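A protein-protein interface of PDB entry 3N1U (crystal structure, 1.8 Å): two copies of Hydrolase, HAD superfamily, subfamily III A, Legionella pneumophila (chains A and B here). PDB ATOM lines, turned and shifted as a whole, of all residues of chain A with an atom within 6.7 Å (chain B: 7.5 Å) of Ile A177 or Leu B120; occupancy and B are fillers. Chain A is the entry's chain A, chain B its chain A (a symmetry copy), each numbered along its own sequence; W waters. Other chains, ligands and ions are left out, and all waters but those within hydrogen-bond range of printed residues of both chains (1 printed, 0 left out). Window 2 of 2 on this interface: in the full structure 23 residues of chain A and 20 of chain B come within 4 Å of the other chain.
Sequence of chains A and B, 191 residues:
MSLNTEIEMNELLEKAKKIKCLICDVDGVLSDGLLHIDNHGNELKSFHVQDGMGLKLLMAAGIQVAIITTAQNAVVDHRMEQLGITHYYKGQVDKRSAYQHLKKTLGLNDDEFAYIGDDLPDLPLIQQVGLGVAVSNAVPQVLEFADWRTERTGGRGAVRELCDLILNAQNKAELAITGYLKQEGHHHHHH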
ATOM      1  N   MET A  53     -34.181  -5.942  23.881  1.00  0.00           N
ATOM      2  CA  MET A  53     -32.898  -6.656  23.705  1.00  0.00           C
ATOM      3  C   MET A  53     -31.866  -6.217  24.758  1.00  0.00           C
ATOM      4  O   MET A  53     -31.147  -7.068  25.297  1.00  0.00           O
ATOM      5  CB  MET A  53     -32.355  -6.427  22.272  1.00  0.00           C
ATOM      6  CG  MET A  53     -30.953  -6.913  22.045  1.00  0.00           C
ATOM      7  SD  MET A  53     -30.975  -8.885  22.038  1.00  0.00           S
ATOM      8  CE  MET A  53     -31.757  -9.010  20.296  1.00  0.00           C
ATOM      9  N   LEU A  57     -30.036  -8.646  27.303  1.00  0.00           N
ATOM     10  CA  LEU A  57     -28.575  -8.753  27.370  1.00  0.00           C
ATOM     11  C   LEU A  57     -28.082  -8.567  28.798  1.00  0.00           C
ATOM     12  O   LEU A  57     -27.135  -9.251  29.228  1.00  0.00           O
ATOM     13  CB  LEU A  57     -27.908  -7.727  26.462  1.00  0.00           C
ATOM     14  CG  LEU A  57     -28.047  -7.982  24.932  1.00  0.00           C
ATOM     15  CD1 LEU A  57     -27.616  -6.781  24.048  1.00  0.00           C
ATOM     16  CD2 LEU A  57     -27.275  -9.201  24.522  1.00  0.00           C
ATOM     17  N   ALA A  60     -28.777 -11.870  30.507  1.00  0.00           N
ATOM     18  CA  ALA A  60     -27.871 -12.919  30.015  1.00  0.00           C
ATOM     19  C   ALA A  60     -26.490 -12.785  30.638  1.00  0.00           C
ATOM     20  O   ALA A  60     -25.800 -13.784  30.790  1.00  0.00           O
ATOM     21  CB  ALA A  60     -27.761 -12.882  28.450  1.00  0.00           C
ATOM     22  N   ARG A 160     -31.768   0.951  26.019  1.00  0.00           N
ATOM     23  CA  ARG A 160     -30.710   0.128  25.418  1.00  0.00           C
ATOM     24  C   ARG A 160     -29.345   0.850  25.584  1.00  0.00           C
ATOM     25  O   ARG A 160     -28.315   0.213  25.842  1.00  0.00           O
ATOM     26  CB  ARG A 160     -30.964  -0.032  23.901  1.00  0.00           C
ATOM     27  CG  ARG A 160     -29.832  -0.754  23.178  1.00  0.00           C
ATOM     28  CD  ARG A 160     -29.477  -2.116  23.883  1.00  0.00           C
ATOM     29  NE  ARG A 160     -28.569  -2.881  23.054  1.00  0.00           N
ATOM     30  CZ  ARG A 160     -28.958  -3.557  21.961  1.00  0.00           C
ATOM     31  NH1 ARG A 160     -30.247  -3.610  21.618  1.00  0.00           N
ATOM     32  NH2 ARG A 160     -28.060  -4.198  21.202  1.00  0.00           N
ATOM     33  N   ASP A 164     -26.084  -0.870  27.280  1.00  0.00           N
ATOM     34  CA  ASP A 164     -24.793  -0.989  26.580  1.00  0.00           C
ATOM     35  C   ASP A 164     -23.683  -0.295  27.371  1.00  0.00           C
ATOM     36  O   ASP A 164     -22.624  -0.864  27.513  1.00  0.00           O
ATOM     37  CB  ASP A 164     -24.855  -0.421  25.158  1.00  0.00           C
ATOM     38  CG  ASP A 164     -25.606  -1.322  24.185  1.00  0.00           C
ATOM     39  OD1 ASP A 164     -26.077  -2.430  24.585  1.00  0.00           O
ATOM     40  OD2 ASP A 164     -25.744  -0.898  23.006  1.00  0.00           O
ATOM     41  N   LEU A 167     -22.864  -2.736  30.242  1.00  0.00           N
ATOM     42  CA  LEU A 167     -22.165  -3.920  29.763  1.00  0.00           C
ATOM     43  C   LEU A 167     -20.748  -3.591  29.333  1.00  0.00           C
ATOM     44  O   LEU A 167     -19.794  -4.309  29.646  1.00  0.00           O
ATOM     45  CB  LEU A 167     -22.937  -4.575  28.617  1.00  0.00           C
ATOM     46  CG  LEU A 167     -24.281  -5.230  29.033  1.00  0.00           C
ATOM     47  CD1 LEU A 167     -25.040  -5.550  27.750  1.00  0.00           C
ATOM     48  CD2 LEU A 167     -23.987  -6.500  29.808  1.00  0.00           C
ATOM     49  N   LYS A 172     -18.643  -6.954  29.731  1.00  0.00           N
ATOM     50  CA  LYS A 172     -19.598  -8.062  29.635  1.00  0.00           C
ATOM     51  C   LYS A 172     -20.424  -8.071  28.342  1.00  0.00           C
ATOM     52  O   LYS A 172     -21.304  -8.912  28.178  1.00  0.00           O
ATOM     53  CB  LYS A 172     -20.556  -8.072  30.842  1.00  0.00           C
ATOM     54  CG  LYS A 172     -19.910  -8.563  32.126  1.00  0.00           C
ATOM     55  CD  LYS A 172     -20.817  -8.407  33.352  1.00  0.00           C
ATOM     56  CE  LYS A 172     -20.043  -8.934  34.642  1.00  0.00           C
ATOM     57  NZ  LYS A 172     -20.706  -8.270  35.814  1.00  0.00           N
ATOM     58  N   ALA A 173     -20.132  -7.159  27.430  1.00  0.00           N
ATOM     59  CA  ALA A 173     -20.918  -7.058  26.174  1.00  0.00           C
ATOM     60  C   ALA A 173     -20.850  -8.377  25.338  1.00  0.00           C
ATOM     61  O   ALA A 173     -21.902  -8.898  24.890  1.00  0.00           O
ATOM     62  CB  ALA A 173     -20.468  -5.875  25.371  1.00  0.00           C
ATOM     63  N   GLU A 174     -19.648  -8.888  25.116  1.00  0.00           N
ATOM     64  CA  GLU A 174     -19.469 -10.181  24.414  1.00  0.00           C
ATOM     65  C   GLU A 174     -20.134 -11.366  25.147  1.00  0.00           C
ATOM     66  O   GLU A 174     -20.889 -12.114  24.517  1.00  0.00           O
ATOM     67  CB  GLU A 174     -17.993 -10.460  24.082  1.00  0.00           C
ATOM     68  CG  GLU A 174     -17.554  -9.961  22.681  1.00  0.00           C
ATOM     69  CD  GLU A 174     -18.487 -10.413  21.513  1.00  0.00           C
ATOM     70  OE1 GLU A 174     -18.865  -9.557  20.655  1.00  0.00           O
ATOM     71  OE2 GLU A 174     -18.850 -11.615  21.446  1.00  0.00           O
ATOM     72  N   LEU A 175     -19.886 -11.502  26.456  1.00  0.00           N
ATOM     73  CA  LEU A 175     -20.606 -12.474  27.321  1.00  0.00           C
ATOM     74  C   LEU A 175     -22.125 -12.439  27.130  1.00  0.00           C
ATOM     75  O   LEU A 175     -22.762 -13.484  26.908  1.00  0.00           O
ATOM     76  CB  LEU A 175     -20.284 -12.278  28.834  1.00  0.00           C
ATOM     77  CG  LEU A 175     -19.302 -13.187  29.576  1.00  0.00           C
ATOM     78  CD1 LEU A 175     -17.905 -13.113  28.984  1.00  0.00           C
ATOM     79  CD2 LEU A 175     -19.273 -12.867  31.074  1.00  0.00           C
ATOM     80  N   ALA A 176     -22.689 -11.222  27.184  1.00  0.00           N
ATOM     81  CA  ALA A 176     -24.128 -10.990  27.051  1.00  0.00           C
ATOM     82  C   ALA A 176     -24.676 -11.475  25.704  1.00  0.00           C
ATOM     83  O   ALA A 176     -25.643 -12.256  25.683  1.00  0.00           O
ATOM     84  CB  ALA A 176     -24.475  -9.510  27.257  1.00  0.00           C
ATOM     85  N   ILE A 177     -24.076 -11.047  24.596  1.00  0.00           N
ATOM     86  CA  ILE A 177     -24.642 -11.443  23.278  1.00  0.00           C
ATOM     87  C   ILE A 177     -24.451 -12.919  23.033  1.00  0.00           C
ATOM     88  O   ILE A 177     -25.307 -13.579  22.405  1.00  0.00           O
ATOM     89  CB  ILE A 177     -24.145 -10.529  22.101  1.00  0.00           C
ATOM     90  CG1 ILE A 177     -24.898 -10.779  20.772  1.00  0.00           C
ATOM     91  CG2 ILE A 177     -22.620 -10.724  21.859  1.00  0.00           C
ATOM     92  CD1 ILE A 177     -26.451 -10.681  20.831  1.00  0.00           C
ATOM     93  N   THR A 178     -23.312 -13.439  23.505  1.00  0.00           N
ATOM     94  CA  THR A 178     -23.023 -14.862  23.347  1.00  0.00           C
ATOM     95  C   THR A 178     -24.094 -15.648  24.096  1.00  0.00           C
ATOM     96  O   THR A 178     -24.760 -16.483  23.494  1.00  0.00           O
ATOM     97  CB  THR A 178     -21.545 -15.208  23.712  1.00  0.00           C
ATOM     98  OG1 THR A 178     -20.685 -14.529  22.768  1.00  0.00           O
ATOM     99  CG2 THR A 178     -21.317 -16.697  23.569  1.00  0.00           C
ATOM    100  N   GLY A 179     -24.264 -15.333  25.370  1.00  0.00           N
ATOM    101  CA  GLY A 179     -25.274 -15.941  26.238  1.00  0.00           C
ATOM    102  C   GLY A 179     -26.705 -15.813  25.750  1.00  0.00           C
ATOM    103  O   GLY A 179     -27.424 -16.820  25.695  1.00  0.00           O
ATOM    104  N   TYR A 180     -27.114 -14.604  25.336  1.00  0.00           N
ATOM    105  CA  TYR A 180     -28.396 -14.441  24.648  1.00  0.00           C
ATOM    106  C   TYR A 180     -28.590 -15.366  23.441  1.00  0.00           C
ATOM    107  O   TYR A 180     -29.657 -15.969  23.304  1.00  0.00           O
ATOM    108  CB  TYR A 180     -28.615 -12.983  24.197  1.00  0.00           C
ATOM    109  CG  TYR A 180     -29.807 -12.804  23.287  1.00  0.00           C
ATOM    110  CD1 TYR A 180     -31.095 -12.637  23.802  1.00  0.00           C
ATOM    111  CD2 TYR A 180     -29.639 -12.804  21.904  1.00  0.00           C
ATOM    112  CE1 TYR A 180     -32.210 -12.465  22.931  1.00  0.00           C
ATOM    113  CE2 TYR A 180     -30.722 -12.623  21.034  1.00  0.00           C
ATOM    114  CZ  TYR A 180     -32.001 -12.465  21.554  1.00  0.00           C
ATOM    115  OH  TYR A 180     -33.049 -12.307  20.654  1.00  0.00           O
ATOM    116  N   LEU A 181     -27.602 -15.412  22.548  1.00  0.00           N
ATOM    117  CA  LEU A 181     -27.751 -16.096  21.243  1.00  0.00           C
ATOM    118  C   LEU A 181     -27.822 -17.606  21.386  1.00  0.00           C
ATOM    119  O   LEU A 181     -28.148 -18.297  20.431  1.00  0.00           O
ATOM    120  CB  LEU A 181     -26.656 -15.707  20.221  1.00  0.00           C
ATOM    121  CG  LEU A 181     -26.754 -14.344  19.503  1.00  0.00           C
ATOM    122  CD1 LEU A 181     -25.452 -14.021  18.767  1.00  0.00           C
ATOM    123  CD2 LEU A 181     -27.928 -14.235  18.542  1.00  0.00           C
ATOM    124  N   LYS A 182     -27.542 -18.082  22.592  1.00  0.00           N
ATOM    125  CA  LYS A 182     -27.521 -19.496  22.916  1.00  0.00           C
ATOM    126  C   LYS A 182     -28.745 -19.919  23.739  1.00  0.00           C
ATOM    127  O   LYS A 182     -28.688 -20.898  24.475  1.00  0.00           O
ATOM    128  CB  LYS A 182     -26.238 -19.813  23.673  1.00  0.00           C
ATOM    129  CG  LYS A 182     -24.964 -19.483  22.915  1.00  0.00           C
ATOM    130  CD  LYS A 182     -23.751 -20.009  23.694  1.00  0.00           C
ATOM    131  CE  LYS A 182     -22.595 -20.384  22.764  1.00  0.00           C
ATOM    132  NZ  LYS A 182     -21.398 -20.817  23.541  1.00  0.00           N
ATOM    133  N   VAL B  93     -33.630 -16.616  16.372  1.00  0.00           N
ATOM    134  CA  VAL B  93     -32.923 -15.826  17.378  1.00  0.00           C
ATOM    135  C   VAL B  93     -31.487 -15.636  16.896  1.00  0.00           C
ATOM    136  O   VAL B  93     -30.981 -14.510  16.850  1.00  0.00           O
ATOM    137  CB  VAL B  93     -32.924 -16.529  18.755  1.00  0.00           C
ATOM    138  CG1 VAL B  93     -31.820 -15.955  19.654  1.00  0.00           C
ATOM    139  CG2 VAL B  93     -34.315 -16.424  19.398  1.00  0.00           C
ATOM    140  N   ASP B  94     -30.835 -16.754  16.577  1.00  0.00           N
ATOM    141  CA  ASP B  94     -29.631 -16.735  15.744  1.00  0.00           C
ATOM    142  C   ASP B  94     -30.108 -16.948  14.298  1.00  0.00           C
ATOM    143  O   ASP B  94     -30.827 -17.923  14.038  1.00  0.00           O
ATOM    144  CB  ASP B  94     -28.655 -17.849  16.147  1.00  0.00           C
ATOM    145  CG  ASP B  94     -27.268 -17.666  15.527  1.00  0.00           C
ATOM    146  OD1 ASP B  94     -27.133 -17.750  14.285  1.00  0.00           O
ATOM    147  OD2 ASP B  94     -26.297 -17.462  16.286  1.00  0.00           O
ATOM    148  N   LYS B  95     -29.696 -16.047  13.395  1.00  0.00           N
ATOM    149  CA  LYS B  95     -30.225 -15.941  12.014  1.00  0.00           C
ATOM    150  C   LYS B  95     -29.373 -16.659  10.948  1.00  0.00           C
ATOM    151  O   LYS B  95     -29.783 -16.759   9.786  1.00  0.00           O
ATOM    152  CB  LYS B  95     -30.369 -14.463  11.631  1.00  0.00           C
ATOM    153  CG  LYS B  95     -31.408 -13.697  12.527  1.00  0.00           C
ATOM    154  CD  LYS B  95     -31.685 -12.292  11.985  1.00  0.00           C
ATOM    155  CE  LYS B  95     -32.874 -11.648  12.749  1.00  0.00           C
ATOM    156  NZ  LYS B  95     -33.155 -10.290  12.228  1.00  0.00           N
ATOM    157  N   GLY B 117     -30.416  -4.542   8.369  1.00  0.00           N
ATOM    158  CA  GLY B 117     -30.543  -4.964   9.761  1.00  0.00           C
ATOM    159  C   GLY B 117     -30.465  -3.761  10.706  1.00  0.00           C
ATOM    160  O   GLY B 117     -30.069  -2.668  10.301  1.00  0.00           O
ATOM    161  N   ASP B 118     -30.754  -3.983  11.981  1.00  0.00           N
ATOM    162  CA  ASP B 118     -30.582  -2.914  13.004  1.00  0.00           C
ATOM    163  C   ASP B 118     -29.913  -3.346  14.343  1.00  0.00           C
ATOM    164  O   ASP B 118     -29.556  -2.482  15.165  1.00  0.00           O
ATOM    165  CB  ASP B 118     -31.958  -2.307  13.320  1.00  0.00           C
ATOM    166  CG  ASP B 118     -32.795  -3.200  14.226  1.00  0.00           C
ATOM    167  OD1 ASP B 118     -33.108  -4.384  13.884  1.00  0.00           O
ATOM    168  OD2 ASP B 118     -33.198  -2.682  15.298  1.00  0.00           O
ATOM    169  N   ASP B 119     -29.783  -4.661  14.611  1.00  0.00           N
ATOM    170  CA  ASP B 119     -29.343  -5.096  15.959  1.00  0.00           C
ATOM    171  C   ASP B 119     -28.326  -6.269  15.862  1.00  0.00           C
ATOM    172  O   ASP B 119     -28.059  -6.792  14.751  1.00  0.00           O
ATOM    173  CB  ASP B 119     -30.552  -5.403  16.902  1.00  0.00           C
ATOM    174  CG  ASP B 119     -30.249  -5.083  18.390  1.00  0.00           C
ATOM    175  OD1 ASP B 119     -29.068  -5.177  18.798  1.00  0.00           O
ATOM    176  OD2 ASP B 119     -31.196  -4.754  19.156  1.00  0.00           O
ATOM    177  N   LEU B 120     -27.734  -6.654  16.981  1.00  0.00           N
ATOM    178  CA  LEU B 120     -26.578  -7.546  16.966  1.00  0.00           C
ATOM    179  C   LEU B 120     -26.817  -8.881  16.266  1.00  0.00           C
ATOM    180  O   LEU B 120     -25.897  -9.392  15.644  1.00  0.00           O
ATOM    181  CB  LEU B 120     -26.058  -7.745  18.412  1.00  0.00           C
ATOM    182  CG  LEU B 120     -25.816  -6.406  19.136  1.00  0.00           C
ATOM    183  CD1 LEU B 120     -25.415  -6.740  20.586  1.00  0.00           C
ATOM    184  CD2 LEU B 120     -24.684  -5.652  18.454  1.00  0.00           C
ATOM    185  N   PRO B 121     -28.031  -9.462  16.370  1.00  0.00           N
ATOM    186  CA  PRO B 121     -28.189 -10.759  15.647  1.00  0.00           C
ATOM    187  C   PRO B 121     -28.151 -10.661  14.116  1.00  0.00           C
ATOM    188  O   PRO B 121     -27.914 -11.677  13.439  1.00  0.00           O
ATOM    189  CB  PRO B 121     -29.522 -11.310  16.161  1.00  0.00           C
ATOM    190  CG  PRO B 121     -29.787 -10.470  17.530  1.00  0.00           C
ATOM    191  CD  PRO B 121     -29.232  -9.115  17.171  1.00  0.00           C
ATOM    192  N   ASP B 122     -28.272  -9.441  13.590  1.00  0.00           N
ATOM    193  CA  ASP B 122     -28.113  -9.188  12.148  1.00  0.00           C
ATOM    194  C   ASP B 122     -26.647  -9.089  11.727  1.00  0.00           C
ATOM    195  O   ASP B 122     -26.327  -9.208  10.550  1.00  0.00           O
ATOM    196  CB  ASP B 122     -28.822  -7.883  11.763  1.00  0.00           C
ATOM    197  CG  ASP B 122     -30.293  -7.877  12.122  1.00  0.00           C
ATOM    198  OD1 ASP B 122     -31.022  -8.853  11.796  1.00  0.00           O
ATOM    199  OD2 ASP B 122     -30.739  -6.879  12.743  1.00  0.00           O
ATOM    200  N   LEU B 123     -25.766  -8.823  12.685  1.00  0.00           N
ATOM    201  CA  LEU B 123     -24.355  -8.552  12.358  1.00  0.00           C
ATOM    202  C   LEU B 123     -23.628  -9.614  11.490  1.00  0.00           C
ATOM    203  O   LEU B 123     -22.977  -9.259  10.513  1.00  0.00           O
ATOM    204  CB  LEU B 123     -23.543  -8.354  13.655  1.00  0.00           C
ATOM    205  CG  LEU B 123     -23.157  -6.924  13.963  1.00  0.00           C
ATOM    206  CD1 LEU B 123     -22.303  -7.032  15.245  1.00  0.00           C
ATOM    207  CD2 LEU B 123     -22.324  -6.417  12.750  1.00  0.00           C
ATOM    208  N   PRO B 124     -23.727 -10.906  11.846  1.00  0.00           N
ATOM    209  CA  PRO B 124     -23.014 -11.894  11.004  1.00  0.00           C
ATOM    210  C   PRO B 124     -23.548 -11.953   9.572  1.00  0.00           C
ATOM    211  O   PRO B 124     -22.773 -12.240   8.669  1.00  0.00           O
ATOM    212  CB  PRO B 124     -23.304 -13.226  11.703  1.00  0.00           C
ATOM    213  CG  PRO B 124     -23.658 -12.839  13.160  1.00  0.00           C
ATOM    214  CD  PRO B 124     -24.350 -11.529  13.037  1.00  0.00           C
ATOM    215  N   LEU B 125     -24.859 -11.733   9.377  1.00  0.00           N
ATOM    216  CA  LEU B 125     -25.417 -11.678   8.038  1.00  0.00           C
ATOM    217  C   LEU B 125     -24.986 -10.415   7.291  1.00  0.00           C
ATOM    218  O   LEU B 125     -24.581 -10.466   6.125  1.00  0.00           O
ATOM    219  CB  LEU B 125     -26.942 -11.861   8.067  1.00  0.00           C
ATOM    220  CG  LEU B 125     -27.361 -13.237   8.638  1.00  0.00           C
ATOM    221  CD1 LEU B 125     -28.817 -13.422   8.272  1.00  0.00           C
ATOM    222  CD2 LEU B 125     -26.531 -14.363   8.041  1.00  0.00           C
ATOM    223  N   ILE B 126     -25.015  -9.284   7.978  1.00  0.00           N
ATOM    224  CA  ILE B 126     -24.571  -8.040   7.392  1.00  0.00           C
ATOM    225  C   ILE B 126     -23.091  -8.133   6.900  1.00  0.00           C
ATOM    226  O   ILE B 126     -22.755  -7.639   5.834  1.00  0.00           O
ATOM    227  CB  ILE B 126     -24.767  -6.921   8.405  1.00  0.00           C
ATOM    228  CG1 ILE B 126     -26.239  -6.497   8.381  1.00  0.00           C
ATOM    229  CG2 ILE B 126     -23.907  -5.691   8.045  1.00  0.00           C
ATOM    230  CD1 ILE B 126     -26.564  -5.515   9.499  1.00  0.00           C
ATOM    231  N   VAL B 139     -28.127  -0.151  16.114  1.00  0.00           N
ATOM    232  CA  VAL B 139     -27.264  -0.067  17.294  1.00  0.00           C
ATOM    233  C   VAL B 139     -25.824   0.225  16.839  1.00  0.00           C
ATOM    234  O   VAL B 139     -25.453  -0.035  15.670  1.00  0.00           O
ATOM    235  CB  VAL B 139     -27.342  -1.332  18.190  1.00  0.00           C
ATOM    236  CG1 VAL B 139     -28.861  -1.560  18.586  1.00  0.00           C
ATOM    237  CG2 VAL B 139     -26.685  -2.566  17.495  1.00  0.00           C
ATOM    238  N   PRO B 140     -25.010   0.772  17.739  1.00  0.00           N
ATOM    239  CA  PRO B 140     -23.680   1.232  17.296  1.00  0.00           C
ATOM    240  C   PRO B 140     -22.770   0.236  16.511  1.00  0.00           C
ATOM    241  O   PRO B 140     -22.158   0.630  15.487  1.00  0.00           O
ATOM    242  CB  PRO B 140     -23.033   1.699  18.613  1.00  0.00           C
ATOM    243  CG  PRO B 140     -24.253   2.277  19.402  1.00  0.00           C
ATOM    244  CD  PRO B 140     -25.324   1.210  19.128  1.00  0.00           C
ATOM    245  N   GLN B 141     -22.679  -1.020  16.941  1.00  0.00           N
ATOM    246  CA  GLN B 141     -21.875  -2.004  16.204  1.00  0.00           C
ATOM    247  C   GLN B 141     -22.387  -2.286  14.793  1.00  0.00           C
ATOM    248  O   GLN B 141     -21.606  -2.457  13.850  1.00  0.00           O
ATOM    249  CB  GLN B 141     -21.863  -3.315  16.946  1.00  0.00           C
ATOM    250  CG  GLN B 141     -20.806  -3.398  18.011  1.00  0.00           C
ATOM    251  CD  GLN B 141     -20.888  -4.717  18.752  1.00  0.00           C
ATOM    252  OE1 GLN B 141     -20.455  -5.747  18.244  1.00  0.00           O
ATOM    253  NE2 GLN B 141     -21.443  -4.688  19.972  1.00  0.00           N
ATOM    254  N   VAL B 142     -23.710  -2.349  14.638  1.00  0.00           N
ATOM    255  CA  VAL B 142     -24.275  -2.548  13.333  1.00  0.00           C
ATOM    256  C   VAL B 142     -23.967  -1.359  12.413  1.00  0.00           C
ATOM    257  O   VAL B 142     -23.617  -1.569  11.256  1.00  0.00           O
ATOM    258  CB  VAL B 142     -25.811  -2.795  13.422  1.00  0.00           C
ATOM    259  CG1 VAL B 142     -26.430  -2.847  12.017  1.00  0.00           C
ATOM    260  CG2 VAL B 142     -26.054  -4.108  14.213  1.00  0.00           C
HETATM  261  O   HOH W   1     -32.536 -12.241  17.802  1.00  0.00           O
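OD1 of Asp A164 lies within salt-bridge range of NE of Arg A160. The backbone NH (N) of Val B139 lies within hydrogen-bond range of the backbone carbonyl oxygen (O) of Asp B118 (2.9 Å). The backbone NH (N) of Asp B119 sits at hydrogen-bond distance from the side-chain carboxylate (OD2) of Asp B122, at 3.1 Å.
Water W1 bridges the side-chain hydroxyl of Tyr A180 (2.9 Å) and the backbone carbonyl oxygen of Val B93 (2.9 Å).
Among the printed residues, merely in contact across the chains: Met A53 with Asp B119 (3.6 Å), Met A53 with Pro B121 (3.7 Å), Arg A160 with Leu B120 (3.7 Å), Arg A160 with Val B139 (3.8 Å), Ile A177 with Leu B120 (3.8 Å), Tyr A180 with Val B93 (3.8 Å) and Leu A181 with Val B93 (3.5 Å).
Of the 17 printed residues of chain B, 5 touch a printed residue of chain A. Hydrophobic or aromatic side chains of chain A within 4 Å of the printed part of chain B: Met A53, Ile A177, Tyr A180 and Leu A181. Among the printed residues, Asp or Glu carboxylates within 4 Å of a Lys or Arg side-chain nitrogen of the other chain: Arg A160 with Asp B119.
The guanidinium group of Arg A160 lies within salt-bridge range of the side-chain carboxylate of Asp B119.
No position is printed for both chains. Of the 8 pairs that touch across the chains among the printed residues, none has its exchanged pair printed and touching as well.
Of the printed residues of chain B, Arg A160 touches Asp B119, Leu B120 and Val B139. Asp A164 touches none of the printed residues of chain B. No residue of chain B comes within 4 Å of Ala A176. Ile A177 touches one residue of chain B. Printed residues of chain B within 4 Å of Tyr A180: Val B93. Printed residues of chain B within 4 Å of Leu A181: Val B93. Printed residues of chain A within 4 Å of Val B93: Tyr A180 and Leu A181. Of the printed residues of chain A, Asp B119 touches Met A53 (3.6 Å) and Arg A160 (2.8 Å). Of chain A, only Arg A160 and Ile A177 come within 4 Å of Leu B120. Pro B124 touches none of the printed residues of chain A. The nearest residue of chain A that does not touch Leu B120 is Leu A57 (4.1 Å).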
